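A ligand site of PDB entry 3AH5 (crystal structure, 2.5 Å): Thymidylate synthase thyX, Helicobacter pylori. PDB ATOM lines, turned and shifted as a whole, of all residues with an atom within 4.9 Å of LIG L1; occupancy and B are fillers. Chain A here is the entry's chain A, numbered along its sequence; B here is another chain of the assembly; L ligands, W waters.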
ATOM      1  N   ARG A  66      -8.072  14.359   9.972  1.00  0.00           N
ATOM      2  CA  ARG A  66      -8.138  15.780  10.272  1.00  0.00           C
ATOM      3  C   ARG A  66      -6.728  16.318  10.446  1.00  0.00           C
ATOM      4  O   ARG A  66      -6.471  17.495  10.197  1.00  0.00           O
ATOM      5  CB  ARG A  66      -8.981  16.037  11.525  1.00  0.00           C
ATOM      6  CG  ARG A  66     -10.443  16.314  11.167  1.00  0.00           C
ATOM      7  CD  ARG A  66     -11.296  16.492  12.401  1.00  0.00           C
ATOM      8  NE  ARG A  66     -11.039  17.756  13.094  1.00  0.00           N
ATOM      9  CZ  ARG A  66     -11.605  18.908  12.752  1.00  0.00           C
ATOM     10  NH1 ARG A  66     -12.444  18.969  11.725  1.00  0.00           N
ATOM     11  NH2 ARG A  66     -11.346  20.002  13.469  1.00  0.00           N
ATOM     12  N   LEU A  69      -5.800  17.305   7.302  1.00  0.00           N
ATOM     13  CA  LEU A  69      -6.590  18.457   6.880  1.00  0.00           C
ATOM     14  C   LEU A  69      -5.803  19.712   7.274  1.00  0.00           C
ATOM     15  O   LEU A  69      -5.786  20.699   6.551  1.00  0.00           O
ATOM     16  CB  LEU A  69      -7.959  18.464   7.573  1.00  0.00           C
ATOM     17  CG  LEU A  69      -8.872  19.657   7.263  1.00  0.00           C
ATOM     18  CD1 LEU A  69      -9.293  19.607   5.806  1.00  0.00           C
ATOM     19  CD2 LEU A  69     -10.085  19.624   8.150  1.00  0.00           C
ATOM     20  N   SER A  73      -5.210  22.452   4.292  1.00  0.00           N
ATOM     21  CA  SER A  73      -5.747  23.802   4.407  1.00  0.00           C
ATOM     22  C   SER A  73      -4.702  24.896   4.243  1.00  0.00           C
ATOM     23  O   SER A  73      -5.052  26.036   3.941  1.00  0.00           O
ATOM     24  CB  SER A  73      -6.465  23.984   5.738  1.00  0.00           C
ATOM     25  OG  SER A  73      -7.657  23.228   5.772  1.00  0.00           O
ATOM     26  N   VAL A  82     -15.472  21.863   3.844  1.00  0.00           N
ATOM     27  CA  VAL A  82     -15.163  20.740   4.698  1.00  0.00           C
ATOM     28  C   VAL A  82     -16.189  20.368   5.752  1.00  0.00           C
ATOM     29  O   VAL A  82     -16.797  21.231   6.403  1.00  0.00           O
ATOM     30  CB  VAL A  82     -13.829  21.001   5.435  1.00  0.00           C
ATOM     31  CG1 VAL A  82     -13.317  19.716   6.127  1.00  0.00           C
ATOM     32  CG2 VAL A  82     -12.796  21.564   4.455  1.00  0.00           C
ATOM     33  N   LYS A  83     -16.369  19.062   5.919  1.00  0.00           N
ATOM     34  CA  LYS A  83     -17.278  18.520   6.913  1.00  0.00           C
ATOM     35  C   LYS A  83     -16.909  19.191   8.232  1.00  0.00           C
ATOM     36  O   LYS A  83     -15.742  19.200   8.637  1.00  0.00           O
ATOM     37  CB  LYS A  83     -17.058  17.005   7.005  1.00  0.00           C
ATOM     38  CG  LYS A  83     -17.769  16.319   8.151  1.00  0.00           C
ATOM     39  CD  LYS A  83     -17.513  14.797   8.114  1.00  0.00           C
ATOM     40  CE  LYS A  83     -18.207  14.110   9.274  1.00  0.00           C
ATOM     41  NZ  LYS A  83     -17.856  12.657   9.364  1.00  0.00           N
ATOM     42  N   SER A  84     -17.904  19.761   8.905  1.00  0.00           N
ATOM     43  CA  SER A  84     -17.662  20.437  10.166  1.00  0.00           C
ATOM     44  C   SER A  84     -17.937  19.561  11.378  1.00  0.00           C
ATOM     45  O   SER A  84     -19.042  19.037  11.521  1.00  0.00           O
ATOM     46  CB  SER A  84     -18.540  21.689  10.265  1.00  0.00           C
ATOM     47  OG  SER A  84     -18.607  22.151  11.598  1.00  0.00           O
ATOM     48  N   SER A  85     -16.927  19.396  12.234  1.00  0.00           N
ATOM     49  CA  SER A  85     -17.074  18.606  13.451  1.00  0.00           C
ATOM     50  C   SER A  85     -18.041  19.321  14.391  1.00  0.00           C
ATOM     51  O   SER A  85     -18.695  18.694  15.243  1.00  0.00           O
ATOM     52  CB  SER A  85     -15.722  18.395  14.147  1.00  0.00           C
ATOM     53  OG  SER A  85     -15.238  19.587  14.746  1.00  0.00           O
ATOM     54  N   ARG A  86     -18.145  20.638  14.237  1.00  0.00           N
ATOM     55  CA  ARG A  86     -19.037  21.437  15.071  1.00  0.00           C
ATOM     56  C   ARG A  86     -20.494  21.172  14.700  1.00  0.00           C
ATOM     57  O   ARG A  86     -21.363  21.116  15.576  1.00  0.00           O
ATOM     58  CB  ARG A  86     -18.753  22.926  14.906  1.00  0.00           C
ATOM     59  CG  ARG A  86     -17.429  23.415  15.475  1.00  0.00           C
ATOM     60  CD  ARG A  86     -17.294  24.926  15.311  1.00  0.00           C
ATOM     61  NE  ARG A  86     -18.298  25.621  16.110  1.00  0.00           N
ATOM     62  CZ  ARG A  86     -18.848  26.784  15.780  1.00  0.00           C
ATOM     63  NH1 ARG A  86     -18.495  27.399  14.657  1.00  0.00           N
ATOM     64  NH2 ARG A  86     -19.774  27.328  16.564  1.00  0.00           N
ATOM     65  N   TYR A  87     -20.762  20.998  13.416  1.00  0.00           N
ATOM     66  CA  TYR A  87     -22.121  20.779  12.947  1.00  0.00           C
ATOM     67  C   TYR A  87     -22.523  19.314  12.777  1.00  0.00           C
ATOM     68  O   TYR A  87     -23.694  19.013  12.556  1.00  0.00           O
ATOM     69  CB  TYR A  87     -22.357  21.484  11.591  1.00  0.00           C
ATOM     70  CG  TYR A  87     -22.024  22.968  11.544  1.00  0.00           C
ATOM     71  CD1 TYR A  87     -22.237  23.792  12.642  1.00  0.00           C
ATOM     72  CD2 TYR A  87     -21.542  23.561  10.360  1.00  0.00           C
ATOM     73  CE1 TYR A  87     -21.992  25.173  12.583  1.00  0.00           C
ATOM     74  CE2 TYR A  87     -21.290  24.939  10.285  1.00  0.00           C
ATOM     75  CZ  TYR A  87     -21.518  25.742  11.399  1.00  0.00           C
ATOM     76  OH  TYR A  87     -21.281  27.095  11.352  1.00  0.00           O
ATOM     77  N   LYS A 147     -15.556  18.413  20.849  1.00  0.00           N
ATOM     78  CA  LYS A 147     -14.590  18.336  19.746  1.00  0.00           C
ATOM     79  C   LYS A 147     -13.138  18.401  20.251  1.00  0.00           C
ATOM     80  O   LYS A 147     -12.254  17.808  19.653  1.00  0.00           O
ATOM     81  CB  LYS A 147     -14.832  19.457  18.719  1.00  0.00           C
ATOM     82  CG  LYS A 147     -14.506  20.860  19.220  1.00  0.00           C
ATOM     83  CD  LYS A 147     -14.947  21.937  18.232  1.00  0.00           C
ATOM     84  CE  LYS A 147     -13.862  22.297  17.218  1.00  0.00           C
ATOM     85  NZ  LYS A 147     -13.446  21.162  16.341  1.00  0.00           N
ATOM     86  N   GLN B  70      -7.103  24.666  13.077  1.00  0.00           N
ATOM     87  CA  GLN B  70      -7.839  24.109  11.950  1.00  0.00           C
ATOM     88  C   GLN B  70      -8.728  25.174  11.312  1.00  0.00           C
ATOM     89  O   GLN B  70      -8.887  25.211  10.092  1.00  0.00           O
ATOM     90  CB  GLN B  70      -8.686  22.934  12.428  1.00  0.00           C
ATOM     91  CG  GLN B  70      -9.185  21.980  11.357  1.00  0.00           C
ATOM     92  CD  GLN B  70      -8.086  21.087  10.812  1.00  0.00           C
ATOM     93  OE1 GLN B  70      -7.494  21.389   9.767  1.00  0.00           O
ATOM     94  NE2 GLN B  70      -7.794  20.003  11.507  1.00  0.00           N
ATOM     95  N   GLU B  71      -9.305  26.055  12.134  1.00  0.00           N
ATOM     96  CA  GLU B  71     -10.195  27.113  11.643  1.00  0.00           C
ATOM     97  C   GLU B  71      -9.441  28.376  11.233  1.00  0.00           C
ATOM     98  O   GLU B  71      -9.767  28.998  10.223  1.00  0.00           O
ATOM     99  CB  GLU B  71     -11.248  27.458  12.696  1.00  0.00           C
ATOM    100  CG  GLU B  71     -12.140  26.291  13.102  1.00  0.00           C
ATOM    101  CD  GLU B  71     -13.170  26.676  14.154  1.00  0.00           C
ATOM    102  OE1 GLU B  71     -14.027  25.826  14.482  1.00  0.00           O
ATOM    103  OE2 GLU B  71     -13.119  27.815  14.671  1.00  0.00           O
ATOM    104  N   ARG B  74      -7.997  28.584   7.855  1.00  0.00           N
ATOM    105  CA  ARG B  74      -8.903  28.799   6.740  1.00  0.00           C
ATOM    106  C   ARG B  74      -8.932  30.230   6.228  1.00  0.00           C
ATOM    107  O   ARG B  74      -9.450  30.501   5.137  1.00  0.00           O
ATOM    108  CB  ARG B  74     -10.312  28.316   7.093  1.00  0.00           C
ATOM    109  CG  ARG B  74     -10.370  26.804   7.233  1.00  0.00           C
ATOM    110  CD  ARG B  74     -10.016  26.108   5.938  1.00  0.00           C
ATOM    111  NE  ARG B  74     -11.010  26.408   4.912  1.00  0.00           N
ATOM    112  CZ  ARG B  74     -12.194  25.821   4.832  1.00  0.00           C
ATOM    113  NH1 ARG B  74     -12.522  24.899   5.715  1.00  0.00           N
ATOM    114  NH2 ARG B  74     -13.064  26.193   3.889  1.00  0.00           N
ATOM    115  N   ARG B 174     -15.163  36.084  13.123  1.00  0.00           N
ATOM    116  CA  ARG B 174     -14.890  35.330  14.350  1.00  0.00           C
ATOM    117  C   ARG B 174     -15.349  35.901  15.685  1.00  0.00           C
ATOM    118  O   ARG B 174     -15.281  35.213  16.705  1.00  0.00           O
ATOM    119  CB  ARG B 174     -13.391  35.005  14.445  1.00  0.00           C
ATOM    120  CG  ARG B 174     -12.840  34.301  13.213  1.00  0.00           C
ATOM    121  CD  ARG B 174     -13.559  32.986  12.939  1.00  0.00           C
ATOM    122  NE  ARG B 174     -13.104  32.379  11.689  1.00  0.00           N
ATOM    123  CZ  ARG B 174     -13.295  31.103  11.358  1.00  0.00           C
ATOM    124  NH1 ARG B 174     -13.928  30.279  12.195  1.00  0.00           N
ATOM    125  NH2 ARG B 174     -12.863  30.650  10.198  1.00  0.00           N
ATOM    126  N   ALA B 179     -19.353  31.770  15.787  1.00  0.00           N
ATOM    127  CA  ALA B 179     -18.044  31.158  15.792  1.00  0.00           C
ATOM    128  C   ALA B 179     -17.709  30.403  17.078  1.00  0.00           C
ATOM    129  O   ALA B 179     -18.309  30.627  18.131  1.00  0.00           O
ATOM    130  CB  ALA B 179     -16.972  32.223  15.536  1.00  0.00           C
ATOM    131  N   LEU B 180     -16.746  29.503  16.957  1.00  0.00           N
ATOM    132  CA  LEU B 180     -16.293  28.714  18.096  1.00  0.00           C
ATOM    133  C   LEU B 180     -15.844  29.685  19.181  1.00  0.00           C
ATOM    134  O   LEU B 180     -15.176  30.681  18.889  1.00  0.00           O
ATOM    135  CB  LEU B 180     -15.119  27.828  17.672  1.00  0.00           C
ATOM    136  CG  LEU B 180     -14.552  26.867  18.707  1.00  0.00           C
ATOM    137  CD1 LEU B 180     -15.619  25.851  19.092  1.00  0.00           C
ATOM    138  CD2 LEU B 180     -13.331  26.170  18.138  1.00  0.00           C
HETATM  139  N1  LIG L   1     -14.574  25.773   9.886  1.00  0.00           N
HETATM  140  C1  LIG L   1     -14.149  26.982  10.431  1.00  0.00           C
HETATM  141  N2  LIG L   1     -14.853  27.571  11.453  1.00  0.00           N
HETATM  142  C2  LIG L   1     -15.998  27.028  12.000  1.00  0.00           C
HETATM  143  C3  LIG L   1     -16.498  25.796  11.508  1.00  0.00           C
HETATM  144  C4  LIG L   1     -15.724  25.164  10.396  1.00  0.00           C
HETATM  145  O1  LIG L   1     -13.154  27.549  10.005  1.00  0.00           O
HETATM  146  O2  LIG L   1     -16.577  27.596  12.902  1.00  0.00           O
HETATM  147  C5  LIG L   1     -13.816  25.104   8.747  1.00  0.00           C
HETATM  148  C6  LIG L   1     -12.266  24.978   8.812  1.00  0.00           C
HETATM  149  C7  LIG L   1     -11.932  23.470   8.965  1.00  0.00           C
HETATM  150  C8  LIG L   1     -13.320  22.844   9.105  1.00  0.00           C
HETATM  151  O3  LIG L   1     -11.293  23.006   7.778  1.00  0.00           O
HETATM  152  O4  LIG L   1     -14.279  23.752   8.496  1.00  0.00           O
HETATM  153  C9  LIG L   1     -13.538  22.704  10.599  1.00  0.00           C
HETATM  154  O5  LIG L   1     -14.826  22.254  10.880  1.00  0.00           O
HETATM  155  P1  LIG L   1     -14.867  22.189  12.472  1.00  0.00           P
HETATM  156  O6  LIG L   1     -14.487  23.477  13.083  1.00  0.00           O
HETATM  157  O7  LIG L   1     -16.336  21.755  12.933  1.00  0.00           O
HETATM  158  O8  LIG L   1     -13.852  21.045  12.947  1.00  0.00           O
HETATM  159  P1  LG2 L   2      -9.998  34.638   3.859  1.00  0.00           P
HETATM  160  O1  LG2 L   2      -9.959  34.715   5.373  1.00  0.00           O
HETATM  161  O2  LG2 L   2      -9.253  33.512   3.177  1.00  0.00           O
HETATM  162  O3  LG2 L   2      -9.766  35.989   3.296  1.00  0.00           O
HETATM  163  C1  LG2 L   2      -9.712  36.244   1.918  1.00  0.00           C
HETATM  164  C2  LG2 L   2     -10.807  37.175   1.386  1.00  0.00           C
HETATM  165  O4  LG2 L   2     -10.396  37.213  -0.002  1.00  0.00           O
HETATM  166  C3  LG2 L   2     -12.253  36.629   1.381  1.00  0.00           C
HETATM  167  O5  LG2 L   2     -13.140  37.300   2.260  1.00  0.00           O
HETATM  168  C4  LG2 L   2     -12.695  36.750  -0.076  1.00  0.00           C
HETATM  169  O6  LG2 L   2     -13.477  37.889  -0.390  1.00  0.00           O
HETATM  170  C5  LG2 L   2     -11.410  36.705  -0.864  1.00  0.00           C
HETATM  171  N1  LG2 L   2     -10.949  35.388  -1.341  1.00  0.00           N
HETATM  172  C6  LG2 L   2      -9.938  34.594  -0.858  1.00  0.00           C
HETATM  173  N2  LG2 L   2      -9.757  33.472  -1.497  1.00  0.00           N
HETATM  174  C7  LG2 L   2     -10.713  33.521  -2.498  1.00  0.00           C
HETATM  175  C8  LG2 L   2     -11.031  32.599  -3.544  1.00  0.00           C
HETATM  176  N3  LG2 L   2     -10.355  31.452  -3.695  1.00  0.00           N
HETATM  177  N4  LG2 L   2     -12.055  32.924  -4.389  1.00  0.00           N
HETATM  178  C9  LG2 L   2     -12.727  34.102  -4.190  1.00  0.00           C
HETATM  179  N5  LG2 L   2     -12.500  35.040  -3.250  1.00  0.00           N
HETATM  180  C10 LG2 L   2     -11.449  34.659  -2.416  1.00  0.00           C
HETATM  181  N6  LG2 L   2     -15.830  25.921   6.126  1.00  0.00           N
HETATM  182  C11 LG2 L   2     -16.207  24.693   5.738  1.00  0.00           C
HETATM  183  O7  LG2 L   2     -15.579  24.073   4.834  1.00  0.00           O
HETATM  184  N7  LG2 L   2     -17.302  24.066   6.376  1.00  0.00           N
HETATM  185  C12 LG2 L   2     -18.078  24.671   7.389  1.00  0.00           C
HETATM  186  O8  LG2 L   2     -19.032  24.041   7.905  1.00  0.00           O
HETATM  187  C13 LG2 L   2     -17.692  25.996   7.743  1.00  0.00           C
HETATM  188  N8  LG2 L   2     -18.408  26.697   8.751  1.00  0.00           N
HETATM  189  C14 LG2 L   2     -17.950  27.971   9.124  1.00  0.00           C
HETATM  190  C15 LG2 L   2     -18.665  28.696  10.147  1.00  0.00           C
HETATM  191  C16 LG2 L   2     -18.253  29.951  10.567  1.00  0.00           C
HETATM  192  C17 LG2 L   2     -19.071  30.642  11.676  1.00  0.00           C
HETATM  193  C18 LG2 L   2     -17.112  30.565   9.976  1.00  0.00           C
HETATM  194  C19 LG2 L   2     -16.614  31.941  10.392  1.00  0.00           C
HETATM  195  C20 LG2 L   2     -16.394  29.860   8.945  1.00  0.00           C
HETATM  196  C21 LG2 L   2     -16.778  28.583   8.503  1.00  0.00           C
HETATM  197  N9  LG2 L   2     -16.077  27.807   7.454  1.00  0.00           N
HETATM  198  C22 LG2 L   2     -16.546  26.558   7.105  1.00  0.00           C
HETATM  199  C23 LG2 L   2     -14.881  28.236   6.703  1.00  0.00           C
HETATM  200  C24 LG2 L   2     -15.096  29.506   5.966  1.00  0.00           C
HETATM  201  O9  LG2 L   2     -16.231  29.307   5.136  1.00  0.00           O
HETATM  202  C25 LG2 L   2     -13.870  29.913   5.155  1.00  0.00           C
HETATM  203  O10 LG2 L   2     -12.758  30.064   6.013  1.00  0.00           O
HETATM  204  C26 LG2 L   2     -14.149  31.260   4.519  1.00  0.00           C
HETATM  205  O11 LG2 L   2     -15.320  31.147   3.675  1.00  0.00           O
HETATM  206  C27 LG2 L   2     -13.024  31.798   3.671  1.00  0.00           C
HETATM  207  O12 LG2 L   2     -13.571  33.076   3.366  1.00  0.00           O
HETATM  208  P2  LG2 L   2     -12.924  34.261   4.133  1.00  0.00           P
HETATM  209  O13 LG2 L   2     -13.704  35.455   3.838  1.00  0.00           O
HETATM  210  O14 LG2 L   2     -12.716  33.819   5.550  1.00  0.00           O
HETATM  211  O15 LG2 L   2     -11.496  34.393   3.435  1.00  0.00           O
HETATM  212  O   HOH W   1     -15.502  29.306  14.474  1.00  0.00           O
HETATM  213  O   HOH W   2     -11.836  22.577  14.526  1.00  0.00           O
HETATM  214  O   HOH W   3      -8.704  23.115   8.491  1.00  0.00           O
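O7 of LIG L1 sits at hydrogen-bond distance from N of Arg 86 (2.5 Å). NH1 of Arg 86 sits at hydrogen-bond distance from O2 of LIG L1 (2.6 Å). An oxygen (O7) of LIG L1 is in hydrogen-bond range of the backbone NH (N) of Ser 85 (2.5 Å). An oxygen (O8) of LIG L1 sits at hydrogen-bond distance from the side-chain hydroxyl of Ser 85. OG of Ser 84 is in hydrogen-bond range of O7 of LIG L1 (2.7 Å). An oxygen (O8) of LIG L1 is in salt-bridge range of the guanidinium group of Arg 66 (2.8 Å). An oxygen (O6) of LIG L1 sits close to the side-chain carboxylate (OE1) of Glu 71 of chain B, 2.8 Å away. An oxygen (O1) of LIG L1 lies within hydrogen-bond range of the guanidinium group (NH2) of Arg 174 of chain B. NH1 of Arg 74 of chain B is in hydrogen-bond range of O3 of LIG L1, at 3.1 Å. The side-chain amino group of Lys 147 lies within salt-bridge range of an oxygen (O8) of LIG L1 (3.4 Å). O of Arg 74 of chain B sits close to O10 of LG2 L2 (3.4 Å). An oxygen (O7) of LG2 L2 lies within hydrogen-bond range of the guanidinium group (NH1) of Arg 74 of chain B. O7 of LG2 L2 sits at hydrogen-bond distance from N of Val 82 (2.4 Å). N7 of LG2 L2 lies within hydrogen-bond range of O of Val 82 (2.9 Å).
N of Arg 86 lies close to OG of Ser 84 (3.1 Å). The side-chain amino group (NZ) of Lys 147 is in hydrogen-bond range of the side-chain hydroxyl (OG) of Ser 85 (2.9 Å). N of Tyr 87 is in hydrogen-bond range of OG of Ser 84, 3.0 Å away. NE2 of Gln 70 of chain B is in hydrogen-bond range of O of Arg 66 (3.1 Å). The side-chain carboxylate of Glu 71 of chain B is in salt-bridge range of the guanidinium group of Arg 174 of chain B, at 3.6 Å. The backbone carbonyl oxygen (O) of Leu 69 is in hydrogen-bond range of the side-chain hydroxyl (OG) of Ser 73.
Merely in contact with LIG L1: Leu 69, Val 82, Lys 83 and Gln 70 of chain B. Hydrophobic or aromatic side chains that line LIG L1: Leu 69 and Val 82.
Water W1 lies within hydrogen-bond range of O2 of LIG L1 (2.6 Å), N of Leu 180 of chain B (2.8 Å), OE2 of Glu 71 of chain B (2.8 Å) and NH1 of Arg 174 of chain B (2.9 Å). Water W3 lies within hydrogen-bond range of OE1 of Gln 70 of chain B, O3 of LIG L1 and OG of Ser 73. Water W2 lies within hydrogen-bond range of NZ of Lys 147, NH2 of Arg 66 and O8 of LIG L1.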
